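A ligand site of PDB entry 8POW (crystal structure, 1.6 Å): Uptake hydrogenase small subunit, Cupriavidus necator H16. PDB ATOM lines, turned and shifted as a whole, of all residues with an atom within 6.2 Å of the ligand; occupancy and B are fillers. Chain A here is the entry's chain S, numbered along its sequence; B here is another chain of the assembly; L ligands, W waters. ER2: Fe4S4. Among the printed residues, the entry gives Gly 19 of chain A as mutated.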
ATOM      1  N   LEU A  15      21.426   2.314 -19.693  1.00  0.00           N
ATOM      2  CA  LEU A  15      20.143   3.002 -19.852  1.00  0.00           C
ATOM      3  C   LEU A  15      19.911   3.817 -18.606  1.00  0.00           C
ATOM      4  O   LEU A  15      19.865   3.272 -17.504  1.00  0.00           O
ATOM      5  CB  LEU A  15      18.990   2.015 -20.054  1.00  0.00           C
ATOM      6  CG  LEU A  15      18.970   1.283 -21.383  1.00  0.00           C
ATOM      7  CD1 LEU A  15      17.727   0.399 -21.433  1.00  0.00           C
ATOM      8  CD2 LEU A  15      18.980   2.273 -22.540  1.00  0.00           C
ATOM      9  N   GLU A  16      19.757   5.122 -18.774  1.00  0.00           N
ATOM     10  CA  GLU A  16      19.662   6.062 -17.652  1.00  0.00           C
ATOM     11  C   GLU A  16      19.152   7.421 -18.113  1.00  0.00           C
ATOM     12  O   GLU A  16      19.012   7.665 -19.308  1.00  0.00           O
ATOM     13  CB  GLU A  16      21.022   6.212 -16.932  1.00  0.00           C
ATOM     14  CG  GLU A  16      22.258   6.192 -17.805  1.00  0.00           C
ATOM     15  CD  GLU A  16      22.709   7.556 -18.299  1.00  0.00           C
ATOM     16  OE1 GLU A  16      22.701   8.534 -17.522  1.00  0.00           O
ATOM     17  OE2 GLU A  16      23.133   7.664 -19.469  1.00  0.00           O
ATOM     18  N   CYS A  17      18.868   8.294 -17.134  1.00  0.00           N
ATOM     19  CA  CYS A  17      18.456   9.652 -17.420  1.00  0.00           C
ATOM     20  C   CYS A  17      19.539  10.694 -17.119  1.00  0.00           C
ATOM     21  O   CYS A  17      19.350  11.861 -17.410  1.00  0.00           O
ATOM     22  CB  CYS A  17      17.174   9.961 -16.628  1.00  0.00           C
ATOM     23  SG  CYS A  17      17.418  10.544 -14.951  1.00  0.00           S
ATOM     24  N   THR A  18      20.657  10.240 -16.548  1.00  0.00           N
ATOM     25  CA  THR A  18      21.799  11.079 -16.178  1.00  0.00           C
ATOM     26  C   THR A  18      21.551  11.950 -14.941  1.00  0.00           C
ATOM     27  O   THR A  18      22.402  12.779 -14.580  1.00  0.00           O
ATOM     28  CB  THR A  18      22.305  11.866 -17.421  1.00  0.00           C
ATOM     29  OG1 THR A  18      22.346  10.953 -18.517  1.00  0.00           O
ATOM     30  CG2 THR A  18      23.684  12.432 -17.210  1.00  0.00           C
ATOM     31  N   GLY A  19      20.428  11.724 -14.251  1.00  0.00           N
ATOM     32  CA  GLY A  19      20.150  12.423 -13.004  1.00  0.00           C
ATOM     33  C   GLY A  19      21.122  12.076 -11.886  1.00  0.00           C
ATOM     34  O   GLY A  19      21.354  12.881 -10.976  1.00  0.00           O
ATOM     35  N   CYS A  20      21.697  10.878 -11.927  1.00  0.00           N
ATOM     36  CA  CYS A  20      22.681  10.475 -10.918  1.00  0.00           C
ATOM     37  C   CYS A  20      24.008  11.252 -11.101  1.00  0.00           C
ATOM     38  O   CYS A  20      24.592  11.741 -10.114  1.00  0.00           O
ATOM     39  CB  CYS A  20      22.861   8.943 -10.880  1.00  0.00           C
ATOM     40  SG  CYS A  20      21.400   8.038 -10.304  1.00  0.00           S
ATOM     41  N   SER A  21      24.477  11.385 -12.347  1.00  0.00           N
ATOM     42  CA  SER A  21      25.631  12.266 -12.619  1.00  0.00           C
ATOM     43  C   SER A  21      25.359  13.703 -12.160  1.00  0.00           C
ATOM     44  O   SER A  21      26.220  14.330 -11.541  1.00  0.00           O
ATOM     45  CB  SER A  21      25.993  12.314 -14.119  1.00  0.00           C
ATOM     46  OG  SER A  21      26.703  11.162 -14.538  1.00  0.00           O
ATOM     47  N   GLU A  76      26.183   3.960 -13.767  1.00  0.00           N
ATOM     48  CA  GLU A  76      24.937   4.717 -13.782  1.00  0.00           C
ATOM     49  C   GLU A  76      24.071   4.053 -14.850  1.00  0.00           C
ATOM     50  O   GLU A  76      24.546   3.736 -15.934  1.00  0.00           O
ATOM     51  CB  GLU A  76      25.214   6.166 -14.125  1.00  0.00           C
ATOM     52  CG  GLU A  76      24.013   7.089 -14.246  1.00  0.00           C
ATOM     53  CD  GLU A  76      24.411   8.545 -14.212  1.00  0.00           C
ATOM     54  OE1 GLU A  76      25.617   8.849 -14.210  1.00  0.00           O
ATOM     55  OE2 GLU A  76      23.509   9.402 -14.146  1.00  0.00           O
ATOM     56  N   GLY A  77      22.803   3.831 -14.552  1.00  0.00           N
ATOM     57  CA  GLY A  77      21.950   3.138 -15.496  1.00  0.00           C
ATOM     58  C   GLY A  77      22.116   1.634 -15.430  1.00  0.00           C
ATOM     59  O   GLY A  77      22.729   1.098 -14.508  1.00  0.00           O
ATOM     60  N   TRP A 112      25.259   3.189  -8.964  1.00  0.00           N
ATOM     61  CA  TRP A 112      24.687   4.499  -8.684  1.00  0.00           C
ATOM     62  C   TRP A 112      23.196   4.466  -8.936  1.00  0.00           C
ATOM     63  O   TRP A 112      22.749   4.071 -10.032  1.00  0.00           O
ATOM     64  CB  TRP A 112      25.239   5.582  -9.605  1.00  0.00           C
ATOM     65  CG  TRP A 112      26.632   6.087  -9.362  1.00  0.00           C
ATOM     66  CD1 TRP A 112      27.561   6.341 -10.320  1.00  0.00           C
ATOM     67  CD2 TRP A 112      27.232   6.468  -8.111  1.00  0.00           C
ATOM     68  NE1 TRP A 112      28.711   6.843  -9.758  1.00  0.00           N
ATOM     69  CE2 TRP A 112      28.538   6.918  -8.407  1.00  0.00           C
ATOM     70  CE3 TRP A 112      26.804   6.449  -6.774  1.00  0.00           C
ATOM     71  CZ2 TRP A 112      29.422   7.363  -7.406  1.00  0.00           C
ATOM     72  CZ3 TRP A 112      27.679   6.893  -5.800  1.00  0.00           C
ATOM     73  CH2 TRP A 112      28.979   7.332  -6.117  1.00  0.00           C
ATOM     74  N   GLY A 113      22.429   4.868  -7.929  1.00  0.00           N
ATOM     75  CA  GLY A 113      21.020   5.105  -8.090  1.00  0.00           C
ATOM     76  C   GLY A 113      20.141   3.870  -8.239  1.00  0.00           C
ATOM     77  O   GLY A 113      20.625   2.727  -8.292  1.00  0.00           O
ATOM     78  N   SER A 114      18.841   4.125  -8.334  1.00  0.00           N
ATOM     79  CA  SER A 114      17.877   3.039  -8.490  1.00  0.00           C
ATOM     80  C   SER A 114      18.048   2.281  -9.819  1.00  0.00           C
ATOM     81  O   SER A 114      17.799   1.085  -9.883  1.00  0.00           O
ATOM     82  CB  SER A 114      16.465   3.595  -8.311  1.00  0.00           C
ATOM     83  OG  SER A 114      16.341   4.141  -6.984  1.00  0.00           O
ATOM     84  N   CYS A 115      18.496   2.963 -10.884  1.00  0.00           N
ATOM     85  CA  CYS A 115      18.680   2.288 -12.188  1.00  0.00           C
ATOM     86  C   CYS A 115      19.662   1.136 -12.043  1.00  0.00           C
ATOM     87  O   CYS A 115      19.352  -0.006 -12.363  1.00  0.00           O
ATOM     88  CB  CYS A 115      19.218   3.221 -13.277  1.00  0.00           C
ATOM     89  SG  CYS A 115      18.033   4.292 -14.086  1.00  0.00           S
ATOM     90  N   ALA A 116      20.859   1.456 -11.566  1.00  0.00           N
ATOM     91  CA  ALA A 116      21.894   0.445 -11.454  1.00  0.00           C
ATOM     92  C   ALA A 116      21.606  -0.533 -10.334  1.00  0.00           C
ATOM     93  O   ALA A 116      21.928  -1.710 -10.465  1.00  0.00           O
ATOM     94  CB  ALA A 116      23.274   1.085 -11.288  1.00  0.00           C
ATOM     95  N   CYS A 120      14.886   0.766 -11.801  1.00  0.00           N
ATOM     96  CA  CYS A 120      14.215   2.073 -11.869  1.00  0.00           C
ATOM     97  C   CYS A 120      13.154   2.129 -12.978  1.00  0.00           C
ATOM     98  O   CYS A 120      12.480   1.134 -13.244  1.00  0.00           O
ATOM     99  CB  CYS A 120      15.225   3.227 -11.924  1.00  0.00           C
ATOM    100  SG  CYS A 120      14.554   4.782 -11.271  1.00  0.00           S
ATOM    101  N   VAL A 121      13.001   3.279 -13.619  1.00  0.00           N
ATOM    102  CA  VAL A 121      11.780   3.549 -14.387  1.00  0.00           C
ATOM    103  C   VAL A 121      11.645   2.650 -15.601  1.00  0.00           C
ATOM    104  O   VAL A 121      10.551   2.163 -15.883  1.00  0.00           O
ATOM    105  CB  VAL A 121      11.643   5.052 -14.756  1.00  0.00           C
ATOM    106  CG1 VAL A 121      12.603   5.470 -15.860  1.00  0.00           C
ATOM    107  CG2 VAL A 121      10.190   5.384 -15.103  1.00  0.00           C
ATOM    108  N   GLN A 122      12.748   2.414 -16.307  1.00  0.00           N
ATOM    109  CA  GLN A 122      12.718   1.541 -17.483  1.00  0.00           C
ATOM    110  C   GLN A 122      12.386   0.087 -17.158  1.00  0.00           C
ATOM    111  O   GLN A 122      11.929  -0.637 -18.025  1.00  0.00           O
ATOM    112  CB  GLN A 122      14.012   1.625 -18.323  1.00  0.00           C
ATOM    113  CG  GLN A 122      15.315   1.283 -17.585  1.00  0.00           C
ATOM    114  CD  GLN A 122      15.972   2.470 -16.938  1.00  0.00           C
ATOM    115  OE1 GLN A 122      15.307   3.435 -16.580  1.00  0.00           O
ATOM    116  NE2 GLN A 122      17.293   2.411 -16.775  1.00  0.00           N
ATOM    117  N   GLY A 148      18.099   5.369  -4.956  1.00  0.00           N
ATOM    118  CA  GLY A 148      17.487   6.689  -4.962  1.00  0.00           C
ATOM    119  C   GLY A 148      17.460   7.183  -6.392  1.00  0.00           C
ATOM    120  O   GLY A 148      18.292   6.776  -7.234  1.00  0.00           O
ATOM    121  N   CYS A 149      16.502   8.062  -6.659  1.00  0.00           N
ATOM    122  CA  CYS A 149      16.272   8.546  -8.009  1.00  0.00           C
ATOM    123  C   CYS A 149      16.247  10.082  -8.072  1.00  0.00           C
ATOM    124  O   CYS A 149      15.168  10.691  -8.109  1.00  0.00           O
ATOM    125  CB  CYS A 149      14.965   7.956  -8.552  1.00  0.00           C
ATOM    126  SG  CYS A 149      14.798   8.245 -10.323  1.00  0.00           S
ATOM    127  N   PRO A 150      17.432  10.728  -8.063  1.00  0.00           N
ATOM    128  CA  PRO A 150      18.739  10.141  -7.814  1.00  0.00           C
ATOM    129  C   PRO A 150      19.005  10.068  -6.303  1.00  0.00           C
ATOM    130  O   PRO A 150      18.202  10.541  -5.515  1.00  0.00           O
ATOM    131  CB  PRO A 150      19.685  11.156  -8.454  1.00  0.00           C
ATOM    132  CG  PRO A 150      19.001  12.465  -8.285  1.00  0.00           C
ATOM    133  CD  PRO A 150      17.518  12.192  -8.180  1.00  0.00           C
ATOM    134  N   PRO A 151      20.140   9.469  -5.903  1.00  0.00           N
ATOM    135  CA  PRO A 151      20.536   9.579  -4.498  1.00  0.00           C
ATOM    136  C   PRO A 151      20.920  11.016  -4.158  1.00  0.00           C
ATOM    137  O   PRO A 151      21.203  11.817  -5.060  1.00  0.00           O
ATOM    138  CB  PRO A 151      21.768   8.669  -4.395  1.00  0.00           C
ATOM    139  CG  PRO A 151      21.792   7.884  -5.673  1.00  0.00           C
ATOM    140  CD  PRO A 151      21.112   8.726  -6.713  1.00  0.00           C
ATOM    141  N   PHE A 257       9.735   0.602  -6.701  1.00  0.00           N
ATOM    142  CA  PHE A 257       8.776   1.613  -6.217  1.00  0.00           C
ATOM    143  C   PHE A 257       7.766   2.098  -7.261  1.00  0.00           C
ATOM    144  O   PHE A 257       6.671   2.516  -6.903  1.00  0.00           O
ATOM    145  CB  PHE A 257       9.489   2.805  -5.552  1.00  0.00           C
ATOM    146  CG  PHE A 257      10.151   3.776  -6.497  1.00  0.00           C
ATOM    147  CD1 PHE A 257      11.437   3.562  -6.960  1.00  0.00           C
ATOM    148  CD2 PHE A 257       9.498   4.939  -6.886  1.00  0.00           C
ATOM    149  CE1 PHE A 257      12.061   4.471  -7.809  1.00  0.00           C
ATOM    150  CE2 PHE A 257      10.111   5.856  -7.732  1.00  0.00           C
ATOM    151  CZ  PHE A 257      11.395   5.622  -8.186  1.00  0.00           C
ATOM    152  N   TRP A 258       8.122   2.017  -8.543  1.00  0.00           N
ATOM    153  CA  TRP A 258       7.217   2.414  -9.624  1.00  0.00           C
ATOM    154  C   TRP A 258       6.003   1.503  -9.767  1.00  0.00           C
ATOM    155  O   TRP A 258       4.996   1.922 -10.339  1.00  0.00           O
ATOM    156  CB  TRP A 258       7.945   2.430 -10.977  1.00  0.00           C
ATOM    157  CG  TRP A 258       9.130   3.317 -11.019  1.00  0.00           C
ATOM    158  CD1 TRP A 258      10.434   2.936 -10.889  1.00  0.00           C
ATOM    159  CD2 TRP A 258       9.148   4.752 -11.196  1.00  0.00           C
ATOM    160  NE1 TRP A 258      11.259   4.029 -10.984  1.00  0.00           N
ATOM    161  CE2 TRP A 258      10.507   5.157 -11.173  1.00  0.00           C
ATOM    162  CE3 TRP A 258       8.160   5.716 -11.384  1.00  0.00           C
ATOM    163  CZ2 TRP A 258      10.889   6.484 -11.329  1.00  0.00           C
ATOM    164  CZ3 TRP A 258       8.544   7.047 -11.518  1.00  0.00           C
ATOM    165  CH2 TRP A 258       9.899   7.419 -11.494  1.00  0.00           C
ATOM    166  N   ARG B  53      14.231   3.202 -23.858  1.00  0.00           N
ATOM    167  CA  ARG B  53      13.726   2.660 -22.601  1.00  0.00           C
ATOM    168  C   ARG B  53      12.238   2.343 -22.652  1.00  0.00           C
ATOM    169  O   ARG B  53      11.777   1.439 -21.966  1.00  0.00           O
ATOM    170  CB  ARG B  53      14.020   3.648 -21.450  1.00  0.00           C
ATOM    171  CG  ARG B  53      15.476   3.695 -21.020  1.00  0.00           C
ATOM    172  CD  ARG B  53      15.767   4.865 -20.093  1.00  0.00           C
ATOM    173  NE  ARG B  53      15.573   6.121 -20.810  1.00  0.00           N
ATOM    174  CZ  ARG B  53      15.328   7.304 -20.271  1.00  0.00           C
ATOM    175  NH1 ARG B  53      15.248   7.484 -18.945  1.00  0.00           N
ATOM    176  NH2 ARG B  53      15.128   8.352 -21.068  1.00  0.00           N
ATOM    177  N   ARG B  73      11.594  11.262 -15.267  1.00  0.00           N
ATOM    178  CA  ARG B  73      12.771  10.402 -15.370  1.00  0.00           C
ATOM    179  C   ARG B  73      13.161  10.037 -16.799  1.00  0.00           C
ATOM    180  O   ARG B  73      14.078   9.247 -17.005  1.00  0.00           O
ATOM    181  CB  ARG B  73      12.627   9.139 -14.519  1.00  0.00           C
ATOM    182  CG  ARG B  73      13.014   9.338 -13.065  1.00  0.00           C
ATOM    183  CD  ARG B  73      12.161  10.349 -12.334  1.00  0.00           C
ATOM    184  NE  ARG B  73      12.509  10.324 -10.919  1.00  0.00           N
ATOM    185  CZ  ARG B  73      11.852  10.916  -9.936  1.00  0.00           C
ATOM    186  NH1 ARG B  73      10.725  11.596 -10.173  1.00  0.00           N
ATOM    187  NH2 ARG B  73      12.312  10.804  -8.696  1.00  0.00           N
ATOM    188  N   GLY B  76      17.295  13.543 -16.417  1.00  0.00           N
ATOM    189  CA  GLY B  76      17.751  14.252 -15.242  1.00  0.00           C
ATOM    190  C   GLY B  76      18.587  15.486 -15.491  1.00  0.00           C
ATOM    191  O   GLY B  76      18.944  16.175 -14.528  1.00  0.00           O
ATOM    192  N   PRO B 228      18.456  16.810  -8.563  1.00  0.00           N
ATOM    193  CA  PRO B 228      17.488  16.606  -9.647  1.00  0.00           C
ATOM    194  C   PRO B 228      16.122  16.059  -9.247  1.00  0.00           C
ATOM    195  O   PRO B 228      15.941  15.569  -8.126  1.00  0.00           O
ATOM    196  CB  PRO B 228      18.193  15.564 -10.558  1.00  0.00           C
ATOM    197  CG  PRO B 228      19.641  15.813 -10.327  1.00  0.00           C
ATOM    198  CD  PRO B 228      19.726  16.113  -8.857  1.00  0.00           C
ATOM    199  N   HIS B 229      15.206  16.128 -10.205  1.00  0.00           N
ATOM    200  CA  HIS B 229      13.859  15.556 -10.135  1.00  0.00           C
ATOM    201  C   HIS B 229      12.948  16.130  -9.039  1.00  0.00           C
ATOM    202  O   HIS B 229      12.434  15.379  -8.198  1.00  0.00           O
ATOM    203  CB  HIS B 229      13.910  14.013 -10.081  1.00  0.00           C
ATOM    204  CG  HIS B 229      14.513  13.377 -11.308  1.00  0.00           C
ATOM    205  ND1 HIS B 229      14.379  13.903 -12.572  1.00  0.00           N
ATOM    206  CD2 HIS B 229      15.214  12.231 -11.453  1.00  0.00           C
ATOM    207  CE1 HIS B 229      14.975  13.121 -13.444  1.00  0.00           C
ATOM    208  NE2 HIS B 229      15.508  12.104 -12.795  1.00  0.00           N
HETATM  209  S3  ER2 L   1      18.176   6.289 -10.810  1.00  0.00           S
HETATM  210 FE3  ER2 L   1      15.958   6.667 -11.517  1.00  0.00          FE
HETATM  211 FE4  ER2 L   1      19.513   8.161 -11.527  1.00  0.00          FE
HETATM  212  S4  ER2 L   1      18.050   9.873 -11.456  1.00  0.00           S
HETATM  213  S1  ER2 L   1      19.862   7.794 -13.781  1.00  0.00           S
HETATM  214 FE1  ER2 L   1      17.840   8.902 -13.476  1.00  0.00          FE
HETATM  215 FE2  ER2 L   1      18.201   6.329 -13.091  1.00  0.00          FE
HETATM  216  S2  ER2 L   1      16.191   7.338 -13.675  1.00  0.00           S
HETATM  217  O   HOH W   1      16.365   5.922 -16.800  1.00  0.00           O
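N of Cys 17 lies close to S1 of the ligand, 3.5 Å away.
An iron atom (FE1) of the ligand is bound by the side-chain sulfur (SG) of Cys 17, at 2.2 Å.
The side-chain sulfur (SG) of Cys 20 binds an iron atom (FE4) of the ligand.
A sulfur (S3) of the ligand sits close to the backbone NH (N) of Cys 115, at 3.3 Å.
The side-chain sulfur (SG) of Cys 115 binds an iron atom (FE2) of the ligand, 2.3 Å away.
The side-chain sulfur (SG) of Cys 149 is bound to an iron atom (FE3) of the ligand (2.3 Å).
FE3 of the ligand is bound by SG of Cys 120, 2.4 Å away.
N of Ser 114 lies close to S3 of the ligand, at 3.4 Å.
NE2 of His 229 of chain B sits close to S4 of the ligand (3.6 Å).
The backbone NH of Thr 18 lies close to a sulfur (S1) of the ligand, 3.8 Å away.
O of Gly 148 sits close to S3 of the ligand.
A sulfur (S4) of the ligand lies close to the backbone nitrogen (N) of Pro 150 (3.6 Å).
Residues that only touch the ligand: Gly 19 (3.6 Å), Glu 16 (3.7 Å) and Arg 73 of chain B (3.8 Å).
Of the 28 residues printed, 13 come within 4 Å of the ligand.
The nearest printed residue that does not touch the ligand is Glu 76 of chain A (4.002 Å).
Water W1 lies within hydrogen-bond range of OE1 of Gln 122 (2.7 Å), NH1 of Arg 53 of chain B (2.9 Å), S2 of the ligand (3.4 Å) and N of Cys 17 (3.5 Å).
The side-chain sulfur (SG) of Cys 17 sits close to a ring nitrogen (NE2) of His 229 of chain B, 3.3 Å away.
SG of Cys 17 sits close to N of Gly 19.
O of Cys 17 is in hydrogen-bond range of N of Gly 76 of chain B.
N of Cys 20 lies within hydrogen-bond range of OE2 of Glu 76 of chain A, at 3.2 Å.
SG of Cys 115 sits close to NE2 of Gln 122, 3.4 Å away.
The backbone carbonyl oxygen (O) of Cys 149 sits at hydrogen-bond distance from the guanidinium group (NH2) of Arg 73 of chain B, at 2.9 Å.
N of Ser 114 sits at hydrogen-bond distance from O of Gly 148, at 2.9 Å.
The side-chain carboxylate (OE1) of Glu 16 sits at hydrogen-bond distance from the side-chain hydroxyl (OG1) of Thr 18 (2.6 Å).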
